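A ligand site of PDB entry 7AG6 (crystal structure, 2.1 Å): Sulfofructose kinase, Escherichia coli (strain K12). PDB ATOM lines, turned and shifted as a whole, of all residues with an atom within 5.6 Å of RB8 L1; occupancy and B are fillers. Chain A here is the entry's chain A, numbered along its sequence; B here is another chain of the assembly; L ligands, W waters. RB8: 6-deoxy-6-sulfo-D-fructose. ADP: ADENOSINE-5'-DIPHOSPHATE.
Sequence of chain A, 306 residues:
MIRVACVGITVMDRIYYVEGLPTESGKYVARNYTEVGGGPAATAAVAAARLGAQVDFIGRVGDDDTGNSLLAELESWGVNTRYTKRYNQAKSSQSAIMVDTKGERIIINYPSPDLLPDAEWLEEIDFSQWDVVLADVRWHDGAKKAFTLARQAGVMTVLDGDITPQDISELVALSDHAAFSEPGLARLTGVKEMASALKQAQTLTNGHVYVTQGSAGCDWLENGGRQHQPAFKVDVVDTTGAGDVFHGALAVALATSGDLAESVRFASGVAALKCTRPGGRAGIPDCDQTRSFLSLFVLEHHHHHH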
ATOM      1  N   ILE A   9     -31.354 -28.453 -10.666  1.00  0.00           N
ATOM      2  CA  ILE A   9     -30.341 -29.499 -10.443  1.00  0.00           C
ATOM      3  C   ILE A   9     -29.781 -29.377  -9.024  1.00  0.00           C
ATOM      4  O   ILE A   9     -29.759 -28.263  -8.473  1.00  0.00           O
ATOM      5  CB  ILE A   9     -29.296 -29.441 -11.547  1.00  0.00           C
ATOM      6  CG1 ILE A   9     -28.553 -28.117 -11.580  1.00  0.00           C
ATOM      7  CG2 ILE A   9     -29.973 -29.760 -12.891  1.00  0.00           C
ATOM      8  CD1 ILE A   9     -27.185 -28.231 -12.239  1.00  0.00           C
ATOM      9  N   VAL A  11     -26.294 -31.122  -7.362  1.00  0.00           N
ATOM     10  CA  VAL A  11     -25.050 -31.818  -7.807  1.00  0.00           C
ATOM     11  C   VAL A  11     -24.070 -31.808  -6.653  1.00  0.00           C
ATOM     12  O   VAL A  11     -24.135 -30.870  -5.845  1.00  0.00           O
ATOM     13  CB  VAL A  11     -24.458 -31.152  -9.058  1.00  0.00           C
ATOM     14  CG1 VAL A  11     -25.534 -30.742 -10.048  1.00  0.00           C
ATOM     15  CG2 VAL A  11     -23.582 -29.983  -8.697  1.00  0.00           C
ATOM     16  N   MET A  12     -23.197 -32.801  -6.576  1.00  0.00           N
ATOM     17  CA  MET A  12     -22.104 -32.800  -5.556  1.00  0.00           C
ATOM     18  C   MET A  12     -20.954 -31.980  -6.145  1.00  0.00           C
ATOM     19  O   MET A  12     -20.501 -32.331  -7.256  1.00  0.00           O
ATOM     20  CB  MET A  12     -21.645 -34.212  -5.202  1.00  0.00           C
ATOM     21  CG  MET A  12     -20.699 -34.244  -4.004  1.00  0.00           C
ATOM     22  SD  MET A  12     -21.443 -33.560  -2.467  1.00  0.00           S
ATOM     23  CE  MET A  12     -22.660 -34.796  -2.039  1.00  0.00           C
ATOM     24  N   ASP A  13     -20.579 -30.913  -5.460  1.00  0.00           N
ATOM     25  CA  ASP A  13     -19.416 -30.054  -5.826  1.00  0.00           C
ATOM     26  C   ASP A  13     -18.149 -30.655  -5.236  1.00  0.00           C
ATOM     27  O   ASP A  13     -18.052 -30.831  -3.994  1.00  0.00           O
ATOM     28  CB  ASP A  13     -19.630 -28.592  -5.456  1.00  0.00           C
ATOM     29  CG  ASP A  13     -20.628 -27.860  -6.337  1.00  0.00           C
ATOM     30  OD1 ASP A  13     -21.059 -28.474  -7.361  1.00  0.00           O
ATOM     31  OD2 ASP A  13     -20.956 -26.689  -6.017  1.00  0.00           O
ATOM     32  N   GLY A  37     -22.584 -29.974  -1.331  1.00  0.00           N
ATOM     33  CA  GLY A  37     -23.780 -29.828  -2.184  1.00  0.00           C
ATOM     34  C   GLY A  37     -23.781 -28.507  -2.948  1.00  0.00           C
ATOM     35  O   GLY A  37     -23.406 -27.485  -2.373  1.00  0.00           O
ATOM     36  N   GLY A  38     -24.208 -28.555  -4.213  1.00  0.00           N
ATOM     37  CA  GLY A  38     -24.354 -27.393  -5.107  1.00  0.00           C
ATOM     38  C   GLY A  38     -25.476 -27.593  -6.100  1.00  0.00           C
ATOM     39  O   GLY A  38     -26.335 -28.468  -5.862  1.00  0.00           O
ATOM     40  N   GLY A  39     -25.419 -26.847  -7.202  1.00  0.00           N
ATOM     41  CA  GLY A  39     -26.487 -26.796  -8.219  1.00  0.00           C
ATOM     42  C   GLY A  39     -27.297 -25.512  -8.052  1.00  0.00           C
ATOM     43  O   GLY A  39     -27.642 -25.180  -6.922  1.00  0.00           O
ATOM     44  N   PRO A  40     -27.583 -24.746  -9.119  1.00  0.00           N
ATOM     45  CA  PRO A  40     -28.176 -23.418  -8.944  1.00  0.00           C
ATOM     46  C   PRO A  40     -29.478 -23.440  -8.122  1.00  0.00           C
ATOM     47  O   PRO A  40     -29.477 -22.777  -7.101  1.00  0.00           O
ATOM     48  CB  PRO A  40     -28.338 -22.895 -10.374  1.00  0.00           C
ATOM     49  CG  PRO A  40     -27.218 -23.594 -11.104  1.00  0.00           C
ATOM     50  CD  PRO A  40     -27.219 -24.990 -10.515  1.00  0.00           C
ATOM     51  N   THR A  43     -28.823 -24.694  -4.311  1.00  0.00           N
ATOM     52  CA  THR A  43     -28.137 -23.685  -3.465  1.00  0.00           C
ATOM     53  C   THR A  43     -29.080 -22.502  -3.247  1.00  0.00           C
ATOM     54  O   THR A  43     -29.081 -21.933  -2.132  1.00  0.00           O
ATOM     55  CB  THR A  43     -26.787 -23.308  -4.067  1.00  0.00           C
ATOM     56  OG1 THR A  43     -25.957 -24.464  -3.956  1.00  0.00           O
ATOM     57  CG2 THR A  43     -26.157 -22.123  -3.343  1.00  0.00           C
ATOM     58  N   SER A  95     -19.937 -32.051 -10.135  1.00  0.00           N
ATOM     59  CA  SER A  95     -19.070 -31.059 -10.806  1.00  0.00           C
ATOM     60  C   SER A  95     -17.675 -31.150 -10.208  1.00  0.00           C
ATOM     61  O   SER A  95     -17.573 -31.421  -8.971  1.00  0.00           O
ATOM     62  CB  SER A  95     -19.603 -29.650 -10.652  1.00  0.00           C
ATOM     63  OG  SER A  95     -20.847 -29.473 -11.300  1.00  0.00           O
ATOM     64  N   ILE A  97     -14.735 -28.440  -9.566  1.00  0.00           N
ATOM     65  CA  ILE A  97     -14.615 -26.956  -9.529  1.00  0.00           C
ATOM     66  C   ILE A  97     -13.190 -26.596  -9.089  1.00  0.00           C
ATOM     67  O   ILE A  97     -12.667 -27.206  -8.159  1.00  0.00           O
ATOM     68  CB  ILE A  97     -15.697 -26.341  -8.623  1.00  0.00           C
ATOM     69  CG1 ILE A  97     -17.104 -26.774  -9.041  1.00  0.00           C
ATOM     70  CG2 ILE A  97     -15.555 -24.836  -8.595  1.00  0.00           C
ATOM     71  CD1 ILE A  97     -18.226 -26.215  -8.207  1.00  0.00           C
ATOM     72  N   ARG A 105     -13.432 -19.088 -10.417  1.00  0.00           N
ATOM     73  CA  ARG A 105     -13.684 -20.556 -10.507  1.00  0.00           C
ATOM     74  C   ARG A 105     -13.877 -21.000 -11.971  1.00  0.00           C
ATOM     75  O   ARG A 105     -14.447 -20.247 -12.833  1.00  0.00           O
ATOM     76  CB  ARG A 105     -14.830 -20.942  -9.579  1.00  0.00           C
ATOM     77  CG  ARG A 105     -16.227 -20.864 -10.166  1.00  0.00           C
ATOM     78  CD  ARG A 105     -16.803 -19.474 -10.168  1.00  0.00           C
ATOM     79  NE  ARG A 105     -18.154 -19.490 -10.745  1.00  0.00           N
ATOM     80  CZ  ARG A 105     -18.428 -19.398 -12.058  1.00  0.00           C
ATOM     81  NH1 ARG A 105     -19.685 -19.408 -12.479  1.00  0.00           N
ATOM     82  NH2 ARG A 105     -17.467 -19.248 -12.950  1.00  0.00           N
ATOM     83  N   ILE A 107     -15.816 -24.336 -13.442  1.00  0.00           N
ATOM     84  CA  ILE A 107     -16.773 -25.428 -13.106  1.00  0.00           C
ATOM     85  C   ILE A 107     -16.879 -26.328 -14.330  1.00  0.00           C
ATOM     86  O   ILE A 107     -17.185 -25.820 -15.441  1.00  0.00           O
ATOM     87  CB  ILE A 107     -18.131 -24.839 -12.715  1.00  0.00           C
ATOM     88  CG1 ILE A 107     -18.024 -23.965 -11.460  1.00  0.00           C
ATOM     89  CG2 ILE A 107     -19.154 -25.951 -12.569  1.00  0.00           C
ATOM     90  CD1 ILE A 107     -19.218 -23.076 -11.202  1.00  0.00           C
ATOM     91  N   ASN A 109     -19.254 -29.345 -15.175  1.00  0.00           N
ATOM     92  CA  ASN A 109     -20.432 -30.100 -14.702  1.00  0.00           C
ATOM     93  C   ASN A 109     -20.606 -31.363 -15.564  1.00  0.00           C
ATOM     94  O   ASN A 109     -20.465 -31.283 -16.811  1.00  0.00           O
ATOM     95  CB  ASN A 109     -21.701 -29.262 -14.718  1.00  0.00           C
ATOM     96  CG  ASN A 109     -22.891 -30.069 -14.275  1.00  0.00           C
ATOM     97  OD1 ASN A 109     -23.772 -30.367 -15.090  1.00  0.00           O
ATOM     98  ND2 ASN A 109     -22.911 -30.464 -13.013  1.00  0.00           N
ATOM     99  N   ARG A 138     -30.610 -25.622 -16.084  1.00  0.00           N
ATOM    100  CA  ARG A 138     -29.790 -26.844 -16.275  1.00  0.00           C
ATOM    101  C   ARG A 138     -30.685 -28.102 -16.317  1.00  0.00           C
ATOM    102  O   ARG A 138     -30.160 -29.110 -16.777  1.00  0.00           O
ATOM    103  CB  ARG A 138     -28.687 -26.911 -15.218  1.00  0.00           C
ATOM    104  CG  ARG A 138     -27.749 -25.715 -15.283  1.00  0.00           C
ATOM    105  CD  ARG A 138     -26.788 -25.704 -16.473  1.00  0.00           C
ATOM    106  NE  ARG A 138     -25.954 -26.896 -16.451  1.00  0.00           N
ATOM    107  CZ  ARG A 138     -25.891 -27.807 -17.410  1.00  0.00           C
ATOM    108  NH1 ARG A 138     -26.549 -27.647 -18.561  1.00  0.00           N
ATOM    109  NH2 ARG A 138     -25.141 -28.871 -17.251  1.00  0.00           N
ATOM    110  N   ASP A 162     -28.433 -19.095 -16.362  1.00  0.00           N
ATOM    111  CA  ASP A 162     -26.973 -19.366 -16.470  1.00  0.00           C
ATOM    112  C   ASP A 162     -26.657 -19.839 -17.886  1.00  0.00           C
ATOM    113  O   ASP A 162     -27.607 -19.982 -18.732  1.00  0.00           O
ATOM    114  CB  ASP A 162     -26.423 -20.297 -15.388  1.00  0.00           C
ATOM    115  CG  ASP A 162     -25.104 -19.794 -14.824  1.00  0.00           C
ATOM    116  OD1 ASP A 162     -24.300 -19.183 -15.602  1.00  0.00           O
ATOM    117  OD2 ASP A 162     -24.904 -19.970 -13.613  1.00  0.00           O
ATOM    118  N   ILE A 163     -25.360 -19.952 -18.169  1.00  0.00           N
ATOM    119  CA  ILE A 163     -24.870 -20.588 -19.414  1.00  0.00           C
ATOM    120  C   ILE A 163     -25.245 -22.064 -19.355  1.00  0.00           C
ATOM    121  O   ILE A 163     -25.169 -22.692 -18.283  1.00  0.00           O
ATOM    122  CB  ILE A 163     -23.362 -20.364 -19.643  1.00  0.00           C
ATOM    123  CG1 ILE A 163     -22.933 -20.811 -21.040  1.00  0.00           C
ATOM    124  CG2 ILE A 163     -22.551 -21.071 -18.564  1.00  0.00           C
ATOM    125  CD1 ILE A 163     -21.740 -20.044 -21.605  1.00  0.00           C
ATOM    126  N   THR A 240     -18.008 -19.271  -5.922  1.00  0.00           N
ATOM    127  CA  THR A 240     -18.821 -20.441  -6.331  1.00  0.00           C
ATOM    128  C   THR A 240     -20.213 -20.321  -5.694  1.00  0.00           C
ATOM    129  O   THR A 240     -20.295 -20.248  -4.454  1.00  0.00           O
ATOM    130  CB  THR A 240     -18.178 -21.784  -5.932  1.00  0.00           C
ATOM    131  OG1 THR A 240     -16.911 -21.925  -6.583  1.00  0.00           O
ATOM    132  CG2 THR A 240     -19.043 -22.976  -6.320  1.00  0.00           C
ATOM    133  N   GLY A 241     -21.261 -20.321  -6.515  1.00  0.00           N
ATOM    134  CA  GLY A 241     -22.659 -20.227  -6.039  1.00  0.00           C
ATOM    135  C   GLY A 241     -23.113 -18.798  -5.723  1.00  0.00           C
ATOM    136  O   GLY A 241     -24.248 -18.668  -5.279  1.00  0.00           O
ATOM    137  N   ASP A 244     -26.222 -18.405  -7.515  1.00  0.00           N
ATOM    138  CA  ASP A 244     -27.263 -19.306  -6.975  1.00  0.00           C
ATOM    139  C   ASP A 244     -27.895 -18.617  -5.766  1.00  0.00           C
ATOM    140  O   ASP A 244     -29.144 -18.571  -5.668  1.00  0.00           O
ATOM    141  CB  ASP A 244     -26.678 -20.648  -6.519  1.00  0.00           C
ATOM    142  CG  ASP A 244     -25.840 -21.417  -7.534  1.00  0.00           C
ATOM    143  OD1 ASP A 244     -25.834 -21.030  -8.725  1.00  0.00           O
ATOM    144  OD2 ASP A 244     -25.197 -22.418  -7.112  1.00  0.00           O
ATOM    145  N   LYS B  27     -18.272 -21.670 -16.691  1.00  0.00           N
ATOM    146  CA  LYS B  27     -19.041 -22.926 -16.558  1.00  0.00           C
ATOM    147  C   LYS B  27     -18.924 -23.687 -17.859  1.00  0.00           C
ATOM    148  O   LYS B  27     -19.243 -23.121 -18.908  1.00  0.00           O
ATOM    149  CB  LYS B  27     -20.522 -22.667 -16.258  1.00  0.00           C
ATOM    150  CG  LYS B  27     -20.805 -22.417 -14.799  1.00  0.00           C
ATOM    151  CD  LYS B  27     -22.277 -22.527 -14.473  1.00  0.00           C
ATOM    152  CE  LYS B  27     -22.535 -22.368 -12.995  1.00  0.00           C
ATOM    153  NZ  LYS B  27     -23.985 -22.516 -12.712  1.00  0.00           N
ATOM    154  N   TYR B  28     -18.541 -24.949 -17.761  1.00  0.00           N
ATOM    155  CA  TYR B  28     -18.411 -25.901 -18.889  1.00  0.00           C
ATOM    156  C   TYR B  28     -19.190 -27.165 -18.557  1.00  0.00           C
ATOM    157  O   TYR B  28     -19.359 -27.511 -17.383  1.00  0.00           O
ATOM    158  CB  TYR B  28     -16.944 -26.262 -19.133  1.00  0.00           C
ATOM    159  CG  TYR B  28     -16.056 -25.061 -19.317  1.00  0.00           C
ATOM    160  CD1 TYR B  28     -15.604 -24.333 -18.233  1.00  0.00           C
ATOM    161  CD2 TYR B  28     -15.654 -24.667 -20.586  1.00  0.00           C
ATOM    162  CE1 TYR B  28     -14.786 -23.231 -18.381  1.00  0.00           C
ATOM    163  CE2 TYR B  28     -14.808 -23.571 -20.757  1.00  0.00           C
ATOM    164  CZ  TYR B  28     -14.387 -22.858 -19.649  1.00  0.00           C
ATOM    165  OH  TYR B  28     -13.583 -21.763 -19.781  1.00  0.00           O
HETATM  166  O1  RB8 L   1     -22.491 -25.907 -13.975  1.00  0.00           O
HETATM  167  S1  RB8 L   1     -23.792 -26.153 -13.455  1.00  0.00           S
HETATM  168  O2  RB8 L   1     -24.690 -25.014 -13.376  1.00  0.00           O
HETATM  169  O3  RB8 L   1     -24.433 -27.315 -14.152  1.00  0.00           O
HETATM  170  C1  RB8 L   1     -23.660 -26.822 -11.822  1.00  0.00           C
HETATM  171  C2  RB8 L   1     -22.788 -25.981 -10.929  1.00  0.00           C
HETATM  172  O4  RB8 L   1     -23.377 -24.684 -10.746  1.00  0.00           O
HETATM  173  C3  RB8 L   1     -23.303 -24.266  -9.375  1.00  0.00           C
HETATM  174  O5  RB8 L   1     -24.555 -24.337  -8.716  1.00  0.00           O
HETATM  175  C4  RB8 L   1     -22.663 -22.870  -9.297  1.00  0.00           C
HETATM  176  O6  RB8 L   1     -23.509 -21.833  -9.840  1.00  0.00           O
HETATM  177  C5  RB8 L   1     -22.390 -25.286  -8.675  1.00  0.00           C
HETATM  178  O7  RB8 L   1     -22.621 -25.372  -7.282  1.00  0.00           O
HETATM  179  C6  RB8 L   1     -22.608 -26.536  -9.518  1.00  0.00           C
HETATM  180  O8  RB8 L   1     -21.505 -27.414  -9.553  1.00  0.00           O
HETATM  181  PB  ADP L   2     -22.741 -16.456 -11.329  1.00  0.00           P
HETATM  182  O1B ADP L   2     -22.013 -17.094 -10.149  1.00  0.00           O
HETATM  183  O2B ADP L   2     -24.074 -17.116 -11.666  1.00  0.00           O
HETATM  184  O3B ADP L   2     -21.873 -16.299 -12.562  1.00  0.00           O
HETATM  185  PA  ADP L   2     -22.194 -13.658 -10.556  1.00  0.00           P
HETATM  186  O1A ADP L   2     -20.731 -13.951 -10.535  1.00  0.00           O
HETATM  187  O2A ADP L   2     -22.673 -12.643 -11.544  1.00  0.00           O
HETATM  188  O3A ADP L   2     -23.077 -14.975 -10.778  1.00  0.00           O
HETATM  189  O5' ADP L   2     -22.628 -13.251  -9.071  1.00  0.00           O
HETATM  190  C5' ADP L   2     -23.991 -12.814  -8.803  1.00  0.00           C
HETATM  191  C4' ADP L   2     -24.002 -11.675  -7.814  1.00  0.00           C
HETATM  192  O4' ADP L   2     -23.291 -12.064  -6.607  1.00  0.00           O
HETATM  193  C3' ADP L   2     -23.332 -10.366  -8.251  1.00  0.00           C
HETATM  194  O3' ADP L   2     -24.193  -9.593  -9.090  1.00  0.00           O
HETATM  195  C2' ADP L   2     -23.048  -9.741  -6.883  1.00  0.00           C
HETATM  196  O2' ADP L   2     -24.225  -9.190  -6.342  1.00  0.00           O
HETATM  197  C1' ADP L   2     -22.556 -10.964  -6.092  1.00  0.00           C
HETATM  198  N9  ADP L   2     -21.135 -11.231  -6.292  1.00  0.00           N
HETATM  199  C8  ADP L   2     -20.567 -12.072  -7.219  1.00  0.00           C
HETATM  200  N7  ADP L   2     -19.261 -12.038  -7.230  1.00  0.00           N
HETATM  201  C5  ADP L   2     -18.944 -11.137  -6.234  1.00  0.00           C
HETATM  202  C6  ADP L   2     -17.707 -10.658  -5.756  1.00  0.00           C
HETATM  203  N6  ADP L   2     -16.534 -11.034  -6.257  1.00  0.00           N
HETATM  204  N1  ADP L   2     -17.733  -9.737  -4.780  1.00  0.00           N
HETATM  205  C2  ADP L   2     -18.919  -9.364  -4.284  1.00  0.00           C
HETATM  206  N3  ADP L   2     -20.145  -9.728  -4.666  1.00  0.00           N
HETATM  207  C4  ADP L   2     -20.088 -10.624  -5.654  1.00  0.00           C
HETATM  208  O   HOH W   1     -20.948 -19.818  -9.455  1.00  0.00           O
HETATM  209  O   HOH W   2     -23.675 -23.895  -5.100  1.00  0.00           O
HETATM  210  O   HOH W   3     -21.985 -26.179 -16.439  1.00  0.00           O
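O7 of RB8 L1 sits at hydrogen-bond distance from OD2 of Asp 13. The side-chain carboxylate (OD2) of Asp 244 lies within hydrogen-bond range of an oxygen (O5) of RB8 L1, at 2.6 Å. The side-chain amino group of Lys 27 of chain B is in salt-bridge range of an oxygen (O2) of RB8 L1 (2.7 Å). The side-chain hydroxyl of Ser 95 is in hydrogen-bond range of an oxygen (O8) of RB8 L1 (2.8 Å). An oxygen (O3) of RB8 L1 is in salt-bridge range of the guanidinium group of Arg 138, at 2.8 Å. An oxygen (O5) of RB8 L1 is in hydrogen-bond range of the backbone NH (N) of Gly 39, at 3.1 Å. An oxygen (O3) of RB8 L1 lies close to the side-chain amide oxygen of Asn 109 (3.3 Å). An oxygen (O3B) of ADP L2 lies within salt-bridge range of the guanidinium group of Arg 105 (3.8 Å).
The side-chain amino group of Lys 27 of chain B is in salt-bridge range of the side-chain carboxylate of Asp 162 (2.9 Å). The side-chain amide nitrogen (ND2) of Asn 109 is in hydrogen-bond range of the side-chain hydroxyl (OG) of Ser 95 (2.9 Å). N of Ser 95 sits at hydrogen-bond distance from O of Met 12. The guanidinium group (NH2) of Arg 138 is in hydrogen-bond range of the side-chain amide oxygen (OD1) of Asn 109 (3.0 Å). O of Gly 39 is in hydrogen-bond range of OG1 of Thr 43. The backbone carbonyl oxygen (O) of Tyr 28 of chain B sits at hydrogen-bond distance from the backbone NH (N) of Asn 109 (2.9 Å). N of Gly 38 sits at hydrogen-bond distance from O of Val 11 (2.8 Å). O of Ile 107 is in hydrogen-bond range of N of Tyr 28 of chain B, 2.8 Å away.
O5 of RB8 L1 lies close to N of Pro 40, at 3.1 Å. CD1 of Ile 9 touches O3 of RB8 L1, at 3.5 Å. Val 11 touches RB8 L1 (CG2 to O8, 3.4 Å). Gly 38 touches RB8 L1 (CA to O7, 3.4 Å). Ile 97 touches RB8 L1. CG2 of Ile 107 touches O1 of RB8 L1, 3.6 Å away. Hydrophobic or aromatic side chains within 4 Å of RB8 L1: Ile 9, Val 11, Pro 40, Ile 97 and Ile 107. Within 4 Å of RB8 L1: Ile 9, Val 11, Asp 13, Gly 38, Gly 39, Pro 40, Ser 95, Ile 97, Ile 107, Asn 109, Arg 138, Asp 244 and Lys 27 of chain B. The nearest printed residue that does not touch RB8 L1 is Gly 241 (4.03 Å).
Water W3 bridges an oxygen (O1) of RB8 L1 (2.5 Å) and the backbone carbonyl oxygen of Tyr 28 of chain B (3.1 Å). Water W2 lies within hydrogen-bond range of the side-chain hydroxyl (OG1) of Thr 43, an oxygen (O7) of RB8 L1 and the side-chain carboxylate (OD2) of Asp 244. Water W1 lies within hydrogen-bond range of the backbone NH of Gly 241 (3.0 Å), an oxygen (O1B) of ADP L2 (3.0 Å), the guanidinium group of Arg 105 (3.1 Å) and an oxygen (O6) of RB8 L1 (3.3 Å).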
